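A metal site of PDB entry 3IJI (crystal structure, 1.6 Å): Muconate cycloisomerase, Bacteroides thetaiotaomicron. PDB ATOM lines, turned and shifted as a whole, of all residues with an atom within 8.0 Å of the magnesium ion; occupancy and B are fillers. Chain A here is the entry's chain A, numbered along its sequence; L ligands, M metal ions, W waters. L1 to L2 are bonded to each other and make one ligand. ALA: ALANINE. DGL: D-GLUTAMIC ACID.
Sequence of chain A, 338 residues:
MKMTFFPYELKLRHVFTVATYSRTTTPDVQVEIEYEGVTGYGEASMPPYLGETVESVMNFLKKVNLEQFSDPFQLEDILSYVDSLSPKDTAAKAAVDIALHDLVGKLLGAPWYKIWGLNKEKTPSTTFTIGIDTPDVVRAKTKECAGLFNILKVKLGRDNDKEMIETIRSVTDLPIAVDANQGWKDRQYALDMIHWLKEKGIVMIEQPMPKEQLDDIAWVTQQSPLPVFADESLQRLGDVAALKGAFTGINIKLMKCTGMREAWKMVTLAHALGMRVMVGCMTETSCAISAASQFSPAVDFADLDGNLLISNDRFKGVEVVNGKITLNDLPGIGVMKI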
ATOM      1  N   LYS A 153      30.692  -5.164 -19.888  1.00  0.00           N
ATOM      2  CA  LYS A 153      29.914  -4.315 -18.997  1.00  0.00           C
ATOM      3  C   LYS A 153      30.054  -4.812 -17.563  1.00  0.00           C
ATOM      4  O   LYS A 153      30.080  -6.018 -17.312  1.00  0.00           O
ATOM      5  CB  LYS A 153      28.441  -4.329 -19.392  1.00  0.00           C
ATOM      6  CG  LYS A 153      27.548  -3.545 -18.430  1.00  0.00           C
ATOM      7  CD  LYS A 153      26.109  -3.522 -18.913  1.00  0.00           C
ATOM      8  CE  LYS A 153      25.212  -2.760 -17.946  1.00  0.00           C
ATOM      9  NZ  LYS A 153      23.825  -2.654 -18.474  1.00  0.00           N
ATOM     10  N   LYS A 155      28.459  -3.902 -13.657  1.00  0.00           N
ATOM     11  CA  LYS A 155      27.475  -3.161 -12.878  1.00  0.00           C
ATOM     12  C   LYS A 155      28.063  -2.843 -11.513  1.00  0.00           C
ATOM     13  O   LYS A 155      28.123  -3.709 -10.624  1.00  0.00           O
ATOM     14  CB  LYS A 155      26.198  -3.992 -12.751  1.00  0.00           C
ATOM     15  CG  LYS A 155      25.540  -4.241 -14.105  1.00  0.00           C
ATOM     16  CD  LYS A 155      24.508  -5.367 -14.064  1.00  0.00           C
ATOM     17  CE  LYS A 155      23.974  -5.631 -15.465  1.00  0.00           C
ATOM     18  NZ  LYS A 155      23.090  -6.825 -15.538  1.00  0.00           N
ATOM     19  N   VAL A 178      30.915   0.903 -17.585  1.00  0.00           N
ATOM     20  CA  VAL A 178      30.343   0.684 -16.270  1.00  0.00           C
ATOM     21  C   VAL A 178      28.995   1.355 -16.073  1.00  0.00           C
ATOM     22  O   VAL A 178      28.740   2.450 -16.587  1.00  0.00           O
ATOM     23  CB  VAL A 178      31.288   1.200 -15.149  1.00  0.00           C
ATOM     24  CG1 VAL A 178      32.620   0.458 -15.203  1.00  0.00           C
ATOM     25  CG2 VAL A 178      31.510   2.695 -15.319  1.00  0.00           C
ATOM     26  N   ASP A 179      28.123   0.680 -15.339  1.00  0.00           N
ATOM     27  CA  ASP A 179      26.809   1.212 -15.024  1.00  0.00           C
ATOM     28  C   ASP A 179      26.756   1.226 -13.491  1.00  0.00           C
ATOM     29  O   ASP A 179      26.685   0.174 -12.858  1.00  0.00           O
ATOM     30  CB  ASP A 179      25.698   0.314 -15.565  1.00  0.00           C
ATOM     31  CG  ASP A 179      24.326   0.946 -15.415  1.00  0.00           C
ATOM     32  OD1 ASP A 179      24.183   1.816 -14.542  1.00  0.00           O
ATOM     33  OD2 ASP A 179      23.405   0.562 -16.168  1.00  0.00           O
ATOM     34  N   ALA A 180      26.835   2.421 -12.910  1.00  0.00           N
ATOM     35  CA  ALA A 180      26.823   2.571 -11.460  1.00  0.00           C
ATOM     36  C   ALA A 180      25.429   2.382 -10.867  1.00  0.00           C
ATOM     37  O   ALA A 180      25.284   2.196  -9.653  1.00  0.00           O
ATOM     38  CB  ALA A 180      27.380   3.937 -11.082  1.00  0.00           C
ATOM     39  N   ASN A 181      24.401   2.443 -11.709  1.00  0.00           N
ATOM     40  CA  ASN A 181      23.037   2.276 -11.254  1.00  0.00           C
ATOM     41  C   ASN A 181      22.708   3.170 -10.053  1.00  0.00           C
ATOM     42  O   ASN A 181      22.189   2.689  -9.045  1.00  0.00           O
ATOM     43  CB  ASN A 181      22.789   0.804 -10.873  1.00  0.00           C
ATOM     44  CG  ASN A 181      22.783  -0.109 -12.087  1.00  0.00           C
ATOM     45  OD1 ASN A 181      21.868  -0.045 -12.909  1.00  0.00           O
ATOM     46  ND2 ASN A 181      23.800  -0.956 -12.200  1.00  0.00           N
ATOM     47  N   GLN A 182      23.006   4.457 -10.173  1.00  0.00           N
ATOM     48  CA  GLN A 182      22.730   5.419  -9.118  1.00  0.00           C
ATOM     49  C   GLN A 182      23.399   5.052  -7.794  1.00  0.00           C
ATOM     50  O   GLN A 182      23.018   5.570  -6.741  1.00  0.00           O
ATOM     51  CB  GLN A 182      21.217   5.531  -8.892  1.00  0.00           C
ATOM     52  CG  GLN A 182      20.431   5.965 -10.119  1.00  0.00           C
ATOM     53  CD  GLN A 182      18.936   5.871  -9.896  1.00  0.00           C
ATOM     54  OE1 GLN A 182      18.374   4.772  -9.843  1.00  0.00           O
ATOM     55  NE2 GLN A 182      18.276   7.013  -9.769  1.00  0.00           N
ATOM     56  N   GLU A 206      27.827   5.146 -16.804  1.00  0.00           N
ATOM     57  CA  GLU A 206      26.376   5.242 -16.910  1.00  0.00           C
ATOM     58  C   GLU A 206      25.728   5.475 -15.542  1.00  0.00           C
ATOM     59  O   GLU A 206      26.057   4.805 -14.564  1.00  0.00           O
ATOM     60  CB  GLU A 206      25.828   3.962 -17.551  1.00  0.00           C
ATOM     61  CG  GLU A 206      24.313   3.887 -17.685  1.00  0.00           C
ATOM     62  CD  GLU A 206      23.858   2.605 -18.372  1.00  0.00           C
ATOM     63  OE1 GLU A 206      22.649   2.309 -18.338  1.00  0.00           O
ATOM     64  OE2 GLU A 206      24.709   1.903 -18.964  1.00  0.00           O
ATOM     65  N   GLN A 207      24.823   6.454 -15.498  1.00  0.00           N
ATOM     66  CA  GLN A 207      24.075   6.822 -14.291  1.00  0.00           C
ATOM     67  C   GLN A 207      24.878   6.691 -12.997  1.00  0.00           C
ATOM     68  O   GLN A 207      24.560   5.878 -12.137  1.00  0.00           O
ATOM     69  CB  GLN A 207      22.813   5.963 -14.186  1.00  0.00           C
ATOM     70  CG  GLN A 207      21.736   6.516 -13.256  1.00  0.00           C
ATOM     71  CD  GLN A 207      21.135   7.807 -13.780  1.00  0.00           C
ATOM     72  OE1 GLN A 207      20.749   7.893 -14.956  1.00  0.00           O
ATOM     73  NE2 GLN A 207      21.031   8.813 -12.916  1.00  0.00           N
ATOM     74  N   PHE A 229      26.508   8.763 -19.355  1.00  0.00           N
ATOM     75  CA  PHE A 229      25.194   8.521 -19.933  1.00  0.00           C
ATOM     76  C   PHE A 229      24.069   8.395 -18.899  1.00  0.00           C
ATOM     77  O   PHE A 229      24.258   7.810 -17.832  1.00  0.00           O
ATOM     78  CB  PHE A 229      25.236   7.248 -20.776  1.00  0.00           C
ATOM     79  CG  PHE A 229      25.930   7.422 -22.089  1.00  0.00           C
ATOM     80  CD1 PHE A 229      25.203   7.689 -23.248  1.00  0.00           C
ATOM     81  CD2 PHE A 229      27.306   7.321 -22.173  1.00  0.00           C
ATOM     82  CE1 PHE A 229      25.842   7.856 -24.464  1.00  0.00           C
ATOM     83  CE2 PHE A 229      27.966   7.483 -23.384  1.00  0.00           C
ATOM     84  CZ  PHE A 229      27.232   7.746 -24.533  1.00  0.00           C
ATOM     85  N   ALA A 230      22.915   8.943 -19.244  1.00  0.00           N
ATOM     86  CA  ALA A 230      21.748   8.893 -18.365  1.00  0.00           C
ATOM     87  C   ALA A 230      20.877   7.694 -18.687  1.00  0.00           C
ATOM     88  O   ALA A 230      20.661   7.364 -19.855  1.00  0.00           O
ATOM     89  CB  ALA A 230      20.940  10.179 -18.525  1.00  0.00           C
ATOM     90  N   ASP A 231      20.381   7.032 -17.647  1.00  0.00           N
ATOM     91  CA  ASP A 231      19.498   5.874 -17.824  1.00  0.00           C
ATOM     92  C   ASP A 231      18.258   6.097 -16.970  1.00  0.00           C
ATOM     93  O   ASP A 231      17.217   6.510 -17.468  1.00  0.00           O
ATOM     94  CB  ASP A 231      20.213   4.582 -17.395  1.00  0.00           C
ATOM     95  CG  ASP A 231      19.390   3.346 -17.708  1.00  0.00           C
ATOM     96  OD1 ASP A 231      18.196   3.489 -18.055  1.00  0.00           O
ATOM     97  OD2 ASP A 231      19.938   2.218 -17.618  1.00  0.00           O
ATOM     98  N   GLU A 232      18.359   5.831 -15.669  1.00  0.00           N
ATOM     99  CA  GLU A 232      17.224   6.028 -14.768  1.00  0.00           C
ATOM    100  C   GLU A 232      16.759   7.486 -14.776  1.00  0.00           C
ATOM    101  O   GLU A 232      15.619   7.782 -14.419  1.00  0.00           O
ATOM    102  CB  GLU A 232      17.597   5.616 -13.337  1.00  0.00           C
ATOM    103  CG  GLU A 232      17.688   4.116 -13.078  1.00  0.00           C
ATOM    104  CD  GLU A 232      18.764   3.435 -13.910  1.00  0.00           C
ATOM    105  OE1 GLU A 232      19.871   3.993 -14.023  1.00  0.00           O
ATOM    106  OE2 GLU A 232      18.497   2.333 -14.434  1.00  0.00           O
ATOM    107  N   ASN A 251      20.483   7.001 -22.586  1.00  0.00           N
ATOM    108  CA  ASN A 251      20.309   5.589 -22.861  1.00  0.00           C
ATOM    109  C   ASN A 251      18.844   5.382 -23.213  1.00  0.00           C
ATOM    110  O   ASN A 251      17.958   5.797 -22.474  1.00  0.00           O
ATOM    111  CB  ASN A 251      20.663   4.755 -21.623  1.00  0.00           C
ATOM    112  CG  ASN A 251      20.698   3.265 -21.914  1.00  0.00           C
ATOM    113  OD1 ASN A 251      20.277   2.816 -22.981  1.00  0.00           O
ATOM    114  ND2 ASN A 251      21.185   2.480 -20.960  1.00  0.00           N
ATOM    115  N   LYS A 253      15.726   2.683 -24.176  1.00  0.00           N
ATOM    116  CA  LYS A 253      15.259   1.307 -24.092  1.00  0.00           C
ATOM    117  C   LYS A 253      13.808   1.304 -24.560  1.00  0.00           C
ATOM    118  O   LYS A 253      12.989   2.092 -24.091  1.00  0.00           O
ATOM    119  CB  LYS A 253      15.351   0.785 -22.650  1.00  0.00           C
ATOM    120  CG  LYS A 253      16.768   0.827 -22.083  1.00  0.00           C
ATOM    121  CD  LYS A 253      16.807   0.321 -20.643  1.00  0.00           C
ATOM    122  CE  LYS A 253      18.133   0.692 -19.983  1.00  0.00           C
ATOM    123  NZ  LYS A 253      18.162   0.335 -18.534  1.00  0.00           N
ATOM    124  N   LYS A 256      10.864   1.326 -22.156  1.00  0.00           N
ATOM    125  CA  LYS A 256      10.694   2.552 -21.375  1.00  0.00           C
ATOM    126  C   LYS A 256      10.114   3.697 -22.202  1.00  0.00           C
ATOM    127  O   LYS A 256       9.380   4.539 -21.680  1.00  0.00           O
ATOM    128  CB  LYS A 256      12.039   3.023 -20.812  1.00  0.00           C
ATOM    129  CG  LYS A 256      12.700   2.094 -19.809  1.00  0.00           C
ATOM    130  CD  LYS A 256      14.083   2.592 -19.394  1.00  0.00           C
ATOM    131  CE  LYS A 256      14.027   3.927 -18.665  1.00  0.00           C
ATOM    132  NZ  LYS A 256      15.383   4.353 -18.182  1.00  0.00           N
ATOM    133  N   MET A 278      23.066   5.911 -26.498  1.00  0.00           N
ATOM    134  CA  MET A 278      23.389   4.513 -26.310  1.00  0.00           C
ATOM    135  C   MET A 278      22.029   3.816 -26.246  1.00  0.00           C
ATOM    136  O   MET A 278      21.008   4.454 -25.982  1.00  0.00           O
ATOM    137  CB  MET A 278      24.196   4.275 -25.028  1.00  0.00           C
ATOM    138  CG  MET A 278      23.452   4.435 -23.721  1.00  0.00           C
ATOM    139  SD  MET A 278      24.502   3.945 -22.306  1.00  0.00           S
ATOM    140  CE  MET A 278      24.304   2.158 -22.357  1.00  0.00           C
ATOM    141  N   GLY A 280      19.892   0.276 -24.795  1.00  0.00           N
ATOM    142  CA  GLY A 280      19.954  -0.829 -23.860  1.00  0.00           C
ATOM    143  C   GLY A 280      18.760  -1.742 -24.044  1.00  0.00           C
ATOM    144  O   GLY A 280      18.013  -1.599 -25.016  1.00  0.00           O
ATOM    145  N   CYS A 281      18.566  -2.671 -23.119  1.00  0.00           N
ATOM    146  CA  CYS A 281      17.461  -3.618 -23.225  1.00  0.00           C
ATOM    147  C   CYS A 281      17.196  -4.309 -21.894  1.00  0.00           C
ATOM    148  O   CYS A 281      17.956  -4.182 -20.942  1.00  0.00           O
ATOM    149  CB  CYS A 281      17.801  -4.703 -24.246  1.00  0.00           C
ATOM    150  SG  CYS A 281      19.165  -5.791 -23.726  1.00  0.00           S
ATOM    151  N   ASP A 303      24.011  -2.090 -25.380  1.00  0.00           N
ATOM    152  CA  ASP A 303      23.950  -3.216 -24.473  1.00  0.00           C
ATOM    153  C   ASP A 303      22.718  -3.952 -24.996  1.00  0.00           C
ATOM    154  O   ASP A 303      21.613  -3.779 -24.493  1.00  0.00           O
ATOM    155  CB  ASP A 303      23.740  -2.756 -23.027  1.00  0.00           C
ATOM    156  CG  ASP A 303      23.889  -3.881 -22.019  1.00  0.00           C
ATOM    157  OD1 ASP A 303      24.878  -4.641 -22.129  1.00  0.00           O
ATOM    158  OD2 ASP A 303      23.040  -4.000 -21.117  1.00  0.00           O
HETATM  159  N   ALA L   1      22.287  -6.642 -20.591  1.00  0.00           N
HETATM  160  CA  ALA L   1      20.966  -6.168 -20.167  1.00  0.00           C
HETATM  161  C   ALA L   1      20.905  -5.488 -18.786  1.00  0.00           C
HETATM  162  O   ALA L   1      21.861  -5.540 -18.013  1.00  0.00           O
HETATM  163  CB  ALA L   1      19.996  -7.326 -20.181  1.00  0.00           C
HETATM  164  N   DGL L   2      19.772  -4.846 -18.490  1.00  0.00           N
HETATM  165  CA  DGL L   2      19.580  -4.175 -17.193  1.00  0.00           C
HETATM  166  C   DGL L   2      19.435  -2.640 -17.313  1.00  0.00           C
HETATM  167  O   DGL L   2      19.218  -2.008 -16.263  1.00  0.00           O
HETATM  168  CB  DGL L   2      18.378  -4.778 -16.443  1.00  0.00           C
HETATM  169  CG  DGL L   2      17.122  -5.075 -17.279  1.00  0.00           C
HETATM  170  CD  DGL L   2      16.254  -6.167 -16.683  1.00  0.00           C
HETATM  171  OE1 DGL L   2      15.950  -6.112 -15.469  1.00  0.00           O
HETATM  172  OE2 DGL L   2      15.867  -7.077 -17.439  1.00  0.00           O
HETATM  173  OXT DGL L   2      19.555  -2.088 -18.432  1.00  0.00           O
HETATM  174 MG    MG M   1      21.625   1.405 -16.863  1.00  0.00          MG
HETATM  175  O   HOH W   1      21.489  -0.135 -18.170  1.00  0.00           O
HETATM  176  O   HOH W   2      21.887   2.847 -15.360  1.00  0.00           O
HETATM  177  O   HOH W   3      20.429   0.387 -15.535  1.00  0.00           O
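The backbone carbonyl oxygen of Cys 281 lies within hydrogen-bond range of a nitrogen (N) of DGL L2, at 3.1 Å.
NZ of Lys 253 lies within salt-bridge range of OXT of DGL L2, at 2.8 Å.
The side-chain amino group (NZ) of Lys 155 lies within hydrogen-bond range of an oxygen (O) of ALA L1.
A nitrogen (N) of ALA L1 lies within salt-bridge range of the side-chain carboxylate (OD2) of Asp 303 (2.8 Å).
The side-chain carboxylate (OD1) of Asp 179 is in hydrogen-bond range of the backbone NH (N) of Asn 181 (2.9 Å).
The backbone NH of Asp 231 is in hydrogen-bond range of the side-chain amide oxygen of Gln 207 (2.8 Å).
The backbone NH (N) of Ala 180 lies within hydrogen-bond range of the backbone carbonyl oxygen (O) of Glu 206 (3.0 Å).
The side-chain carboxylate (OD1) of Asp 231 lies within salt-bridge range of the side-chain amino group (NZ) of Lys 256, at 2.9 Å.
OD2 of Asp 179 sits close to NZ of Lys 153 (3.98 Å).
The side-chain carboxylate (OD1) of Asp 231 lies within salt-bridge range of the side-chain amino group (NZ) of Lys 253, 3.2 Å away.
O of Val 178 sits at hydrogen-bond distance from N of Glu 206 (2.9 Å).
ND2 of Asn 251 lies close to OE1 of Glu 206, 3.0 Å away.
NZ of Lys 253 touches the magnesium ion (3.99 Å).
Four residues have an atom within 4 Å of the magnesium ion: Asp 179, Glu 206, Asp 231 and Lys 253.
Along chain A the residues within 4 Å of the magnesium ion span positions 179 to 253.
The nearest printed residue that does not touch the magnesium ion is Glu 232 (4.1 Å).
The magnesium ion is bound by OE1 of Glu 206 (2.0 Å), OD2 of Asp 231 (2.0 Å), water W1 (2.0 Å), water W3 (2.1 Å), OD2 of Asp 179 (2.1 Å) and water W2 (2.1 Å).
The magnesium ion has six donor atoms within binding distance.
Water W2 lies within hydrogen-bond range of the side-chain carboxylate (OD1) of Asp 179 (2.6 Å) and the side-chain carboxylate (OE1) of Glu 232 (2.7 Å).
Water W3 lies within hydrogen-bond range of an oxygen (O) of DGL L2 (2.8 Å), the side-chain carboxylate of Glu 232 (3.0 Å) and the side-chain amide oxygen of Asn 181 (3.0 Å).
Water W1 lies within hydrogen-bond range of an oxygen (OXT) of DGL L2 (2.8 Å), the side-chain amino group (NZ) of Lys 253 (3.4 Å) and the side-chain amino group (NZ) of Lys 153 (3.4 Å).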
